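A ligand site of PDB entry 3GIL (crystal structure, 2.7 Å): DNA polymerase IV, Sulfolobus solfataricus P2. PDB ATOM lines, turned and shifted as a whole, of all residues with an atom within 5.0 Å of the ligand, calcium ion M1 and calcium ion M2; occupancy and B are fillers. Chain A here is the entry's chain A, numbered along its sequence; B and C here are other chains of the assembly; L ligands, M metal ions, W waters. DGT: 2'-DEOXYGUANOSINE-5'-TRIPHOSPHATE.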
ATOM      1  N   ASP A   7     -16.908   1.351   2.627  1.00  0.00           N
ATOM      2  CA  ASP A   7     -17.255   2.273   3.725  1.00  0.00           C
ATOM      3  C   ASP A   7     -18.578   1.836   4.328  1.00  0.00           C
ATOM      4  O   ASP A   7     -19.633   1.974   3.714  1.00  0.00           O
ATOM      5  CB  ASP A   7     -17.330   3.712   3.196  1.00  0.00           C
ATOM      6  CG  ASP A   7     -17.793   4.721   4.266  1.00  0.00           C
ATOM      7  OD1 ASP A   7     -18.810   4.425   4.935  1.00  0.00           O
ATOM      8  OD2 ASP A   7     -17.198   5.825   4.380  1.00  0.00           O
ATOM      9  N   PHE A   8     -18.529   1.345   5.556  1.00  0.00           N
ATOM     10  CA  PHE A   8     -19.688   0.736   6.202  1.00  0.00           C
ATOM     11  C   PHE A   8     -20.841   1.747   6.411  1.00  0.00           C
ATOM     12  O   PHE A   8     -20.593   2.953   6.594  1.00  0.00           O
ATOM     13  CB  PHE A   8     -19.297   0.068   7.539  1.00  0.00           C
ATOM     14  CG  PHE A   8     -17.946  -0.682   7.523  1.00  0.00           C
ATOM     15  CD1 PHE A   8     -17.477  -1.316   6.400  1.00  0.00           C
ATOM     16  CD2 PHE A   8     -17.176  -0.759   8.694  1.00  0.00           C
ATOM     17  CE1 PHE A   8     -16.280  -2.000   6.430  1.00  0.00           C
ATOM     18  CE2 PHE A   8     -15.995  -1.432   8.712  1.00  0.00           C
ATOM     19  CZ  PHE A   8     -15.545  -2.065   7.583  1.00  0.00           C
ATOM     20  N   ASP A   9     -22.083   1.266   6.377  1.00  0.00           N
ATOM     21  CA  ASP A   9     -23.271   2.140   6.469  1.00  0.00           C
ATOM     22  C   ASP A   9     -23.614   2.484   7.931  1.00  0.00           C
ATOM     23  O   ASP A   9     -23.696   1.592   8.792  1.00  0.00           O
ATOM     24  CB  ASP A   9     -24.507   1.497   5.811  1.00  0.00           C
ATOM     25  CG  ASP A   9     -24.308   1.179   4.312  1.00  0.00           C
ATOM     26  OD1 ASP A   9     -23.471   1.833   3.668  1.00  0.00           O
ATOM     27  OD2 ASP A   9     -25.018   0.282   3.785  1.00  0.00           O
ATOM     28  N   TYR A  10     -23.856   3.761   8.190  1.00  0.00           N
ATOM     29  CA  TYR A  10     -24.256   4.281   9.510  1.00  0.00           C
ATOM     30  C   TYR A  10     -23.728   3.452  10.680  1.00  0.00           C
ATOM     31  O   TYR A  10     -24.450   3.076  11.618  1.00  0.00           O
ATOM     32  CB  TYR A  10     -25.779   4.489   9.564  1.00  0.00           C
ATOM     33  CG  TYR A  10     -26.622   3.268   9.377  1.00  0.00           C
ATOM     34  CD1 TYR A  10     -27.317   2.711  10.453  1.00  0.00           C
ATOM     35  CD2 TYR A  10     -26.801   2.685   8.119  1.00  0.00           C
ATOM     36  CE1 TYR A  10     -28.133   1.611  10.303  1.00  0.00           C
ATOM     37  CE2 TYR A  10     -27.615   1.559   7.951  1.00  0.00           C
ATOM     38  CZ  TYR A  10     -28.265   1.021   9.060  1.00  0.00           C
ATOM     39  OH  TYR A  10     -29.077  -0.080   8.964  1.00  0.00           O
ATOM     40  N   PHE A  11     -22.414   3.238  10.614  1.00  0.00           N
ATOM     41  CA  PHE A  11     -21.754   2.132  11.279  1.00  0.00           C
ATOM     42  C   PHE A  11     -22.129   1.947  12.745  1.00  0.00           C
ATOM     43  O   PHE A  11     -22.657   0.897  13.109  1.00  0.00           O
ATOM     44  CB  PHE A  11     -20.231   2.230  11.094  1.00  0.00           C
ATOM     45  CG  PHE A  11     -19.469   1.037  11.603  1.00  0.00           C
ATOM     46  CD1 PHE A  11     -19.838  -0.251  11.229  1.00  0.00           C
ATOM     47  CD2 PHE A  11     -18.391   1.201  12.447  1.00  0.00           C
ATOM     48  CE1 PHE A  11     -19.165  -1.337  11.698  1.00  0.00           C
ATOM     49  CE2 PHE A  11     -17.700   0.113  12.922  1.00  0.00           C
ATOM     50  CZ  PHE A  11     -18.078  -1.155  12.554  1.00  0.00           C
ATOM     51  N   TYR A  12     -21.893   2.942  13.604  1.00  0.00           N
ATOM     52  CA  TYR A  12     -22.148   2.715  15.038  1.00  0.00           C
ATOM     53  C   TYR A  12     -23.608   2.324  15.263  1.00  0.00           C
ATOM     54  O   TYR A  12     -23.886   1.321  15.926  1.00  0.00           O
ATOM     55  CB  TYR A  12     -21.811   3.907  15.901  1.00  0.00           C
ATOM     56  CG  TYR A  12     -20.354   4.273  15.942  1.00  0.00           C
ATOM     57  CD1 TYR A  12     -19.418   3.664  15.128  1.00  0.00           C
ATOM     58  CD2 TYR A  12     -19.930   5.294  16.792  1.00  0.00           C
ATOM     59  CE1 TYR A  12     -18.105   4.059  15.169  1.00  0.00           C
ATOM     60  CE2 TYR A  12     -18.620   5.681  16.838  1.00  0.00           C
ATOM     61  CZ  TYR A  12     -17.714   5.082  16.023  1.00  0.00           C
ATOM     62  OH  TYR A  12     -16.416   5.476  16.074  1.00  0.00           O
ATOM     63  N   VAL A  32     -22.190  10.813  22.167  1.00  0.00           N
ATOM     64  CA  VAL A  32     -21.046  10.971  23.002  1.00  0.00           C
ATOM     65  C   VAL A  32     -21.437  11.941  24.091  1.00  0.00           C
ATOM     66  O   VAL A  32     -21.455  13.136  23.876  1.00  0.00           O
ATOM     67  CB  VAL A  32     -19.875  11.558  22.208  1.00  0.00           C
ATOM     68  CG1 VAL A  32     -18.643  11.609  23.083  1.00  0.00           C
ATOM     69  CG2 VAL A  32     -19.650  10.758  20.947  1.00  0.00           C
ATOM     70  N   VAL A  43     -23.596  14.145  18.806  1.00  0.00           N
ATOM     71  CA  VAL A  43     -23.986  12.863  18.201  1.00  0.00           C
ATOM     72  C   VAL A  43     -22.836  12.283  17.394  1.00  0.00           C
ATOM     73  O   VAL A  43     -22.190  13.008  16.680  1.00  0.00           O
ATOM     74  CB  VAL A  43     -25.221  13.044  17.306  1.00  0.00           C
ATOM     75  CG1 VAL A  43     -25.517  11.783  16.547  1.00  0.00           C
ATOM     76  CG2 VAL A  43     -26.409  13.449  18.155  1.00  0.00           C
ATOM     77  N   ALA A  44     -22.572  10.984  17.522  1.00  0.00           N
ATOM     78  CA  ALA A  44     -21.506  10.343  16.748  1.00  0.00           C
ATOM     79  C   ALA A  44     -21.999   9.996  15.352  1.00  0.00           C
ATOM     80  O   ALA A  44     -21.310  10.240  14.358  1.00  0.00           O
ATOM     81  CB  ALA A  44     -21.014   9.090  17.445  1.00  0.00           C
ATOM     82  N   THR A  45     -23.185   9.413  15.294  1.00  0.00           N
ATOM     83  CA  THR A  45     -23.883   9.184  14.060  1.00  0.00           C
ATOM     84  C   THR A  45     -25.361   8.862  14.370  1.00  0.00           C
ATOM     85  O   THR A  45     -25.776   8.847  15.534  1.00  0.00           O
ATOM     86  CB  THR A  45     -23.223   8.062  13.254  1.00  0.00           C
ATOM     87  OG1 THR A  45     -23.889   7.913  11.987  1.00  0.00           O
ATOM     88  CG2 THR A  45     -23.287   6.766  14.015  1.00  0.00           C
ATOM     89  N   TYR A  48     -30.585   6.184   9.111  1.00  0.00           N
ATOM     90  CA  TYR A  48     -31.192   6.970   8.038  1.00  0.00           C
ATOM     91  C   TYR A  48     -32.585   7.460   8.438  1.00  0.00           C
ATOM     92  O   TYR A  48     -32.986   8.574   8.093  1.00  0.00           O
ATOM     93  CB  TYR A  48     -31.135   6.206   6.688  1.00  0.00           C
ATOM     94  CG  TYR A  48     -29.769   6.421   6.052  1.00  0.00           C
ATOM     95  CD1 TYR A  48     -28.643   5.790   6.559  1.00  0.00           C
ATOM     96  CD2 TYR A  48     -29.583   7.351   5.012  1.00  0.00           C
ATOM     97  CE1 TYR A  48     -27.353   6.049   6.014  1.00  0.00           C
ATOM     98  CE2 TYR A  48     -28.323   7.600   4.456  1.00  0.00           C
ATOM     99  CZ  TYR A  48     -27.203   6.953   4.975  1.00  0.00           C
ATOM    100  OH  TYR A  48     -25.954   7.210   4.424  1.00  0.00           O
ATOM    101  N   ARG A  51     -31.920  10.531  10.231  1.00  0.00           N
ATOM    102  CA  ARG A  51     -31.433  11.598   9.338  1.00  0.00           C
ATOM    103  C   ARG A  51     -32.562  12.297   8.568  1.00  0.00           C
ATOM    104  O   ARG A  51     -32.467  13.488   8.262  1.00  0.00           O
ATOM    105  CB  ARG A  51     -30.359  11.074   8.392  1.00  0.00           C
ATOM    106  CG  ARG A  51     -29.031  10.884   9.092  1.00  0.00           C
ATOM    107  CD  ARG A  51     -27.961  10.300   8.168  1.00  0.00           C
ATOM    108  NE  ARG A  51     -27.085   9.386   8.905  1.00  0.00           N
ATOM    109  CZ  ARG A  51     -26.038   8.751   8.395  1.00  0.00           C
ATOM    110  NH1 ARG A  51     -25.676   8.942   7.143  1.00  0.00           N
ATOM    111  NH2 ARG A  51     -25.336   7.936   9.159  1.00  0.00           N
ATOM    112  N   ALA A  57     -24.389  13.161  12.446  1.00  0.00           N
ATOM    113  CA  ALA A  57     -23.104  13.235  13.131  1.00  0.00           C
ATOM    114  C   ALA A  57     -22.738  14.683  13.350  1.00  0.00           C
ATOM    115  O   ALA A  57     -22.829  15.492  12.429  1.00  0.00           O
ATOM    116  CB  ALA A  57     -22.037  12.533  12.328  1.00  0.00           C
ATOM    117  N   GLY A  58     -22.375  15.033  14.561  1.00  0.00           N
ATOM    118  CA  GLY A  58     -21.807  16.322  14.807  1.00  0.00           C
ATOM    119  C   GLY A  58     -22.681  17.257  15.604  1.00  0.00           C
ATOM    120  O   GLY A  58     -22.171  18.051  16.381  1.00  0.00           O
ATOM    121  N   MET A  76     -22.140   5.862  23.121  1.00  0.00           N
ATOM    122  CA  MET A  76     -21.160   5.349  22.213  1.00  0.00           C
ATOM    123  C   MET A  76     -20.253   4.380  22.961  1.00  0.00           C
ATOM    124  O   MET A  76     -19.690   4.728  24.006  1.00  0.00           O
ATOM    125  CB  MET A  76     -20.358   6.519  21.639  1.00  0.00           C
ATOM    126  CG  MET A  76     -19.461   6.161  20.458  1.00  0.00           C
ATOM    127  SD  MET A  76     -18.113   7.348  20.204  1.00  0.00           S
ATOM    128  CE  MET A  76     -17.308   7.291  21.808  1.00  0.00           C
ATOM    129  N   SER A 103     -10.256   4.698   8.484  1.00  0.00           N
ATOM    130  CA  SER A 103     -11.027   5.090   9.650  1.00  0.00           C
ATOM    131  C   SER A 103     -11.567   3.834  10.294  1.00  0.00           C
ATOM    132  O   SER A 103     -11.412   2.735   9.756  1.00  0.00           O
ATOM    133  CB  SER A 103     -12.204   5.970   9.244  1.00  0.00           C
ATOM    134  OG  SER A 103     -13.325   5.190   8.864  1.00  0.00           O
ATOM    135  N   ILE A 104     -12.253   4.000  11.426  1.00  0.00           N
ATOM    136  CA  ILE A 104     -12.872   2.847  12.063  1.00  0.00           C
ATOM    137  C   ILE A 104     -13.841   2.085  11.113  1.00  0.00           C
ATOM    138  O   ILE A 104     -14.106   0.898  11.355  1.00  0.00           O
ATOM    139  CB  ILE A 104     -13.583   3.227  13.368  1.00  0.00           C
ATOM    140  CG1 ILE A 104     -13.873   1.952  14.184  1.00  0.00           C
ATOM    141  CG2 ILE A 104     -14.850   4.034  13.082  1.00  0.00           C
ATOM    142  CD1 ILE A 104     -14.158   2.183  15.645  1.00  0.00           C
ATOM    143  N   ASP A 105     -14.348   2.737  10.065  1.00  0.00           N
ATOM    144  CA  ASP A 105     -15.321   2.089   9.179  1.00  0.00           C
ATOM    145  C   ASP A 105     -15.032   2.035   7.680  1.00  0.00           C
ATOM    146  O   ASP A 105     -15.899   1.630   6.932  1.00  0.00           O
ATOM    147  CB  ASP A 105     -16.725   2.678   9.392  1.00  0.00           C
ATOM    148  CG  ASP A 105     -16.991   3.877   8.525  1.00  0.00           C
ATOM    149  OD1 ASP A 105     -16.030   4.677   8.321  1.00  0.00           O
ATOM    150  OD2 ASP A 105     -18.165   4.040   8.061  1.00  0.00           O
ATOM    151  N   GLU A 106     -13.831   2.411   7.232  1.00  0.00           N
ATOM    152  CA  GLU A 106     -13.534   2.339   5.801  1.00  0.00           C
ATOM    153  C   GLU A 106     -12.106   1.868   5.497  1.00  0.00           C
ATOM    154  O   GLU A 106     -11.213   1.979   6.333  1.00  0.00           O
ATOM    155  CB  GLU A 106     -13.802   3.693   5.145  1.00  0.00           C
ATOM    156  CG  GLU A 106     -12.936   4.830   5.653  1.00  0.00           C
ATOM    157  CD  GLU A 106     -13.410   6.189   5.147  1.00  0.00           C
ATOM    158  OE1 GLU A 106     -12.520   7.007   4.772  1.00  0.00           O
ATOM    159  OE2 GLU A 106     -14.650   6.445   5.129  1.00  0.00           O
ATOM    160  N   LYS A 159     -23.956   5.837  -1.363  1.00  0.00           N
ATOM    161  CA  LYS A 159     -24.362   5.593   0.040  1.00  0.00           C
ATOM    162  C   LYS A 159     -25.844   5.353   0.231  1.00  0.00           C
ATOM    163  O   LYS A 159     -26.654   6.035  -0.382  1.00  0.00           O
ATOM    164  CB  LYS A 159     -23.875   6.707   0.997  1.00  0.00           C
ATOM    165  CG  LYS A 159     -22.541   6.381   1.586  1.00  0.00           C
ATOM    166  CD  LYS A 159     -22.006   7.471   2.481  1.00  0.00           C
ATOM    167  CE  LYS A 159     -20.576   7.135   2.928  1.00  0.00           C
ATOM    168  NZ  LYS A 159     -19.875   8.358   3.293  1.00  0.00           N
ATOM    169  N   PRO A 160     -26.181   4.599   1.292  1.00  0.00           N
ATOM    170  CA  PRO A 160     -26.683   3.368   1.794  1.00  0.00           C
ATOM    171  C   PRO A 160     -26.641   2.189   0.842  1.00  0.00           C
ATOM    172  O   PRO A 160     -27.283   2.179  -0.206  1.00  0.00           O
ATOM    173  CB  PRO A 160     -28.142   3.729   2.180  1.00  0.00           C
ATOM    174  CG  PRO A 160     -28.154   5.192   2.297  1.00  0.00           C
ATOM    175  CD  PRO A 160     -26.692   5.601   2.240  1.00  0.00           C
ATOM    176  P    DC B   5     -17.865  19.967  22.094  1.00  0.00           P
ATOM    177  OP1  DC B   5     -18.008  20.626  23.434  1.00  0.00           O
ATOM    178  OP2  DC B   5     -16.775  20.378  21.178  1.00  0.00           O
ATOM    179  O5'  DC B   5     -17.810  18.393  22.324  1.00  0.00           O
ATOM    180  C5'  DC B   5     -18.752  17.771  23.116  1.00  0.00           C
ATOM    181  C4'  DC B   5     -18.444  16.305  23.232  1.00  0.00           C
ATOM    182  O4'  DC B   5     -18.687  15.660  21.946  1.00  0.00           O
ATOM    183  C3'  DC B   5     -16.989  15.968  23.568  1.00  0.00           C
ATOM    184  O3'  DC B   5     -17.010  14.854  24.439  1.00  0.00           O
ATOM    185  C2'  DC B   5     -16.363  15.663  22.197  1.00  0.00           C
ATOM    186  C1'  DC B   5     -17.518  15.076  21.408  1.00  0.00           C
ATOM    187  N1   DC B   5     -17.616  15.402  19.964  1.00  0.00           N
ATOM    188  C2   DC B   5     -17.558  14.350  19.017  1.00  0.00           C
ATOM    189  O2   DC B   5     -17.412  13.186  19.376  1.00  0.00           O
ATOM    190  N3   DC B   5     -17.691  14.639  17.701  1.00  0.00           N
ATOM    191  C4   DC B   5     -17.873  15.899  17.296  1.00  0.00           C
ATOM    192  N4   DC B   5     -17.993  16.071  15.986  1.00  0.00           N
ATOM    193  C5   DC B   5     -17.943  16.983  18.228  1.00  0.00           C
ATOM    194  C6   DC B   5     -17.819  16.695  19.541  1.00  0.00           C
ATOM    195  P   8OG B   6     -15.734  14.522  25.307  1.00  0.00           P
ATOM    196  OP1 8OG B   6     -15.955  13.427  26.317  1.00  0.00           O
ATOM    197  OP2 8OG B   6     -15.249  15.881  25.714  1.00  0.00           O
ATOM    198  O5' 8OG B   6     -14.817  13.920  24.158  1.00  0.00           O
ATOM    199  C5' 8OG B   6     -14.923  12.551  23.720  1.00  0.00           C
ATOM    200  C4' 8OG B   6     -14.043  12.406  22.520  1.00  0.00           C
ATOM    201  O4' 8OG B   6     -14.562  12.793  21.228  1.00  0.00           O
ATOM    202  C3' 8OG B   6     -12.722  12.355  22.506  1.00  0.00           C
ATOM    203  O3' 8OG B   6     -12.176  11.275  22.476  1.00  0.00           O
ATOM    204  C2' 8OG B   6     -12.244  13.462  21.591  1.00  0.00           C
ATOM    205  C1' 8OG B   6     -13.464  13.594  20.726  1.00  0.00           C
ATOM    206  N9  8OG B   6     -13.722  14.434  19.709  1.00  0.00           N
ATOM    207  C8  8OG B   6     -13.890  15.744  19.786  1.00  0.00           C
ATOM    208  N7  8OG B   6     -14.233  16.271  18.599  1.00  0.00           N
ATOM    209  C5  8OG B   6     -14.326  15.211  17.758  1.00  0.00           C
ATOM    210  C6  8OG B   6     -14.652  14.997  16.327  1.00  0.00           C
ATOM    211  O6  8OG B   6     -14.950  15.971  15.596  1.00  0.00           O
ATOM    212  N1  8OG B   6     -14.643  13.728  15.871  1.00  0.00           N
ATOM    213  C2  8OG B   6     -14.345  12.671  16.631  1.00  0.00           C
ATOM    214  N2  8OG B   6     -14.366  11.420  16.114  1.00  0.00           N
ATOM    215  N3  8OG B   6     -14.040  12.792  17.924  1.00  0.00           N
ATOM    216  C4  8OG B   6     -14.026  13.991  18.507  1.00  0.00           C
ATOM    217  O8  8OG B   6     -13.668  16.430  20.853  1.00  0.00           O
ATOM    218  P   2DT C  13     -15.109  11.869   5.337  1.00  0.00           P
ATOM    219  OP1 2DT C  13     -14.558  10.577   4.932  1.00  0.00           O
ATOM    220  OP2 2DT C  13     -15.850  12.786   4.443  1.00  0.00           O
ATOM    221  O5' 2DT C  13     -16.113  11.462   6.515  1.00  0.00           O
ATOM    222  N1  2DT C  13     -15.480  14.279  11.125  1.00  0.00           N
ATOM    223  C6  2DT C  13     -16.059  15.242  10.306  1.00  0.00           C
ATOM    224  C2  2DT C  13     -15.261  14.489  12.459  1.00  0.00           C
ATOM    225  O2  2DT C  13     -14.760  13.628  13.167  1.00  0.00           O
ATOM    226  N3  2DT C  13     -15.664  15.713  12.936  1.00  0.00           N
ATOM    227  C4  2DT C  13     -16.214  16.742  12.187  1.00  0.00           C
ATOM    228  O4  2DT C  13     -16.518  17.813  12.717  1.00  0.00           O
ATOM    229  C5  2DT C  13     -16.444  16.450  10.787  1.00  0.00           C
ATOM    230  C5M 2DT C  13     -17.068  17.510   9.919  1.00  0.00           C
ATOM    231  C2' 2DT C  13     -16.099  11.872  10.810  1.00  0.00           C
ATOM    232  C5' 2DT C  13     -16.308  12.117   7.716  1.00  0.00           C
ATOM    233  C4' 2DT C  13     -15.164  11.772   8.659  1.00  0.00           C
ATOM    234  O4' 2DT C  13     -14.732  12.988   9.302  1.00  0.00           O
ATOM    235  C1' 2DT C  13     -15.048  12.947  10.676  1.00  0.00           C
ATOM    236  C3' 2DT C  13     -15.503  10.881   9.832  1.00  0.00           C
HETATM  237  PG  DGT L   1     -22.627   6.641   6.528  1.00  0.00           P
HETATM  238  O1G DGT L   1     -21.222   6.764   5.961  1.00  0.00           O
HETATM  239  O2G DGT L   1     -23.825   6.408   5.599  1.00  0.00           O
HETATM  240  O3G DGT L   1     -22.729   8.126   6.205  1.00  0.00           O
HETATM  241  O3B DGT L   1     -22.917   7.012   8.070  1.00  0.00           O
HETATM  242  PB  DGT L   1     -21.600   6.795   8.958  1.00  0.00           P
HETATM  243  O1B DGT L   1     -21.012   5.427   8.804  1.00  0.00           O
HETATM  244  O2B DGT L   1     -22.051   6.975  10.388  1.00  0.00           O
HETATM  245  O3A DGT L   1     -20.630   8.004   8.505  1.00  0.00           O
HETATM  246  PA  DGT L   1     -19.046   7.864   8.591  1.00  0.00           P
HETATM  247  O1A DGT L   1     -18.397   9.196   8.336  1.00  0.00           O
HETATM  248  O2A DGT L   1     -18.521   6.908   7.518  1.00  0.00           O
HETATM  249  O5' DGT L   1     -18.581   7.499  10.062  1.00  0.00           O
HETATM  250  C5' DGT L   1     -18.225   6.181  10.458  1.00  0.00           C
HETATM  251  C4' DGT L   1     -18.388   6.185  11.972  1.00  0.00           C
HETATM  252  O4' DGT L   1     -17.512   7.158  12.510  1.00  0.00           O
HETATM  253  C3' DGT L   1     -19.778   6.619  12.404  1.00  0.00           C
HETATM  254  O3' DGT L   1     -20.747   5.555  12.454  1.00  0.00           O
HETATM  255  C2' DGT L   1     -19.504   7.225  13.741  1.00  0.00           C
HETATM  256  C1' DGT L   1     -18.105   7.792  13.621  1.00  0.00           C
HETATM  257  N9  DGT L   1     -18.239   9.232  13.380  1.00  0.00           N
HETATM  258  C8  DGT L   1     -18.558   9.891  12.208  1.00  0.00           C
HETATM  259  N7  DGT L   1     -18.616  11.198  12.337  1.00  0.00           N
HETATM  260  C5  DGT L   1     -18.344  11.416  13.675  1.00  0.00           C
HETATM  261  C6  DGT L   1     -18.282  12.613  14.439  1.00  0.00           C
HETATM  262  O6  DGT L   1     -18.424  13.814  14.116  1.00  0.00           O
HETATM  263  N1  DGT L   1     -17.982  12.335  15.767  1.00  0.00           N
HETATM  264  C2  DGT L   1     -17.772  11.104  16.298  1.00  0.00           C
HETATM  265  N2  DGT L   1     -17.545  11.046  17.589  1.00  0.00           N
HETATM  266  N3  DGT L   1     -17.829   9.999  15.591  1.00  0.00           N
HETATM  267  C4  DGT L   1     -18.122  10.220  14.311  1.00  0.00           C
HETATM  268 CA    CA M   1     -16.502   6.311   6.565  1.00  0.00          CA
HETATM  269 CA    CA M   2     -19.829   5.119   6.847  1.00  0.00          CA
HETATM  270  O   HOH W   1     -22.034   4.365   4.128  1.00  0.00           O
HETATM  271  O   HOH W   2     -14.912   7.518   8.688  1.00  0.00           O
HETATM  272  O   HOH W   3     -24.544   9.261   3.561  1.00  0.00           O
HETATM  273  O   HOH W   4     -16.077   7.816  17.338  1.00  0.00           O
HETATM  274  O   HOH W   5     -19.267  15.377  12.197  1.00  0.00           O
HETATM  275  O   HOH W   6     -22.476  10.298   4.969  1.00  0.00           O
HETATM  276  O   HOH W   7     -16.963   8.282   5.787  1.00  0.00           O
HETATM  277  O   HOH W   8     -22.097  11.105   8.262  1.00  0.00           O
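OG1 of Thr 45 is in hydrogen-bond range of O2B of the ligand, 2.6 Å away. The side-chain amino group of Lys 159 lies close to an oxygen (O1G) of the ligand, 3.4 Å away. O3G of the ligand lies within salt-bridge range of NH1 of Arg 51, at 3.2 Å. N of Tyr 10 lies close to O3B of the ligand. O2G of the ligand is in hydrogen-bond range of OH of Tyr 48. N of Tyr 12 sits at hydrogen-bond distance from O3' of the ligand. The backbone NH of Phe 11 sits at hydrogen-bond distance from an oxygen (O3') of the ligand, at 3.4 Å. O2 of DC 5 of chain B sits at hydrogen-bond distance from a nitrogen (N2) of the ligand (2.8 Å).
The guanidinium group (NH1) of Arg 51 lies within hydrogen-bond range of the side-chain hydroxyl (OH) of Tyr 48 (3.2 Å). The side-chain hydroxyl (OG1) of Thr 45 lies within hydrogen-bond range of the guanidinium group (NH2) of Arg 51 (3.2 Å). N1 of 8OG 6 of chain B sits close to O2 of 2DT 13 of chain C (2.7 Å). The backbone NH (N) of Asp 105 is in hydrogen-bond range of the side-chain hydroxyl (OG) of Ser 103 (2.9 Å). The side-chain amino group of Lys 159 lies close to the side-chain carboxylate of Asp 7, 3.8 Å away. The side-chain hydroxyl (OG) of Ser 103 lies close to the backbone NH (N) of Glu 106 (3.3 Å).
The backbone carbonyl oxygen of Ala 44 lies close to a nitrogen (N9) of the ligand (3.4 Å). Residues that only touch the ligand: 2DT 13 of chain C (3.0 Å), 8OG 6 of chain B (3.4 Å), Ala 57 (3.7 Å) and Val 32 (3.97 Å). Hydrophobic or aromatic side chains that line the ligand: Phe 11, Tyr 12, Val 32, Ala 44, Tyr 48 and Ala 57. 16 residues have an atom within 4 Å of the ligand: Asp 7, Phe 8, Tyr 10, Phe 11, Tyr 12, Val 32, Ala 44, Thr 45, Tyr 48, Arg 51, Ala 57, Asp 105, Lys 159, DC 5 of chain B, 8OG 6 of chain B and 2DT 13 of chain C.
Within 4 Å of calcium ion M1: Asp 7, Asp 105 and Glu 106. The nearest printed residue that does not touch calcium ion M1 is Ser 103 (4.1 Å).
Of the 24 residues printed, 3 come within 4 Å of calcium ion M2. The nearest printed residue that does not touch calcium ion M2 is Tyr 10 (4.5 Å).
Calcium ion M1 is bound by water W7 (2.2 Å). O2A of the ligand binds calcium ion M1, 2.3 Å away. OD2 of Asp 7 is bound to calcium ion M1. Calcium ion M1 is bound by OE2 of Glu 106 (2.3 Å). OD1 of Asp 105 is bound to calcium ion M1. Calcium ion M1 has five donor atoms within binding distance. Slightly farther from calcium ion M1 lies water W2 (2.9 Å).
Calcium ion M2 is bound by the side-chain carboxylate of Asp 7, an oxygen (O1B) of the ligand, the backbone carbonyl oxygen of Phe 8, an oxygen (O2A) of the ligand, the side-chain carboxylate of Asp 105 and an oxygen (O1G) of the ligand. Calcium ion M2 has six donor atoms within binding distance.
Water W7 lies within hydrogen-bond range of O1A of the ligand and O5' of 2DT 13 of chain C. Water W1 lies within hydrogen-bond range of OD1 of Asp 9, O2G of the ligand and O of Asp 7. Water W4 lies within hydrogen-bond range of OH of Tyr 12, N3 of the ligand and SD of Met 76. Water W3 bridges the side-chain hydroxyl (OH) of Tyr 48 (2.6 Å) and an oxygen (O3G) of the ligand (3.4 Å).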
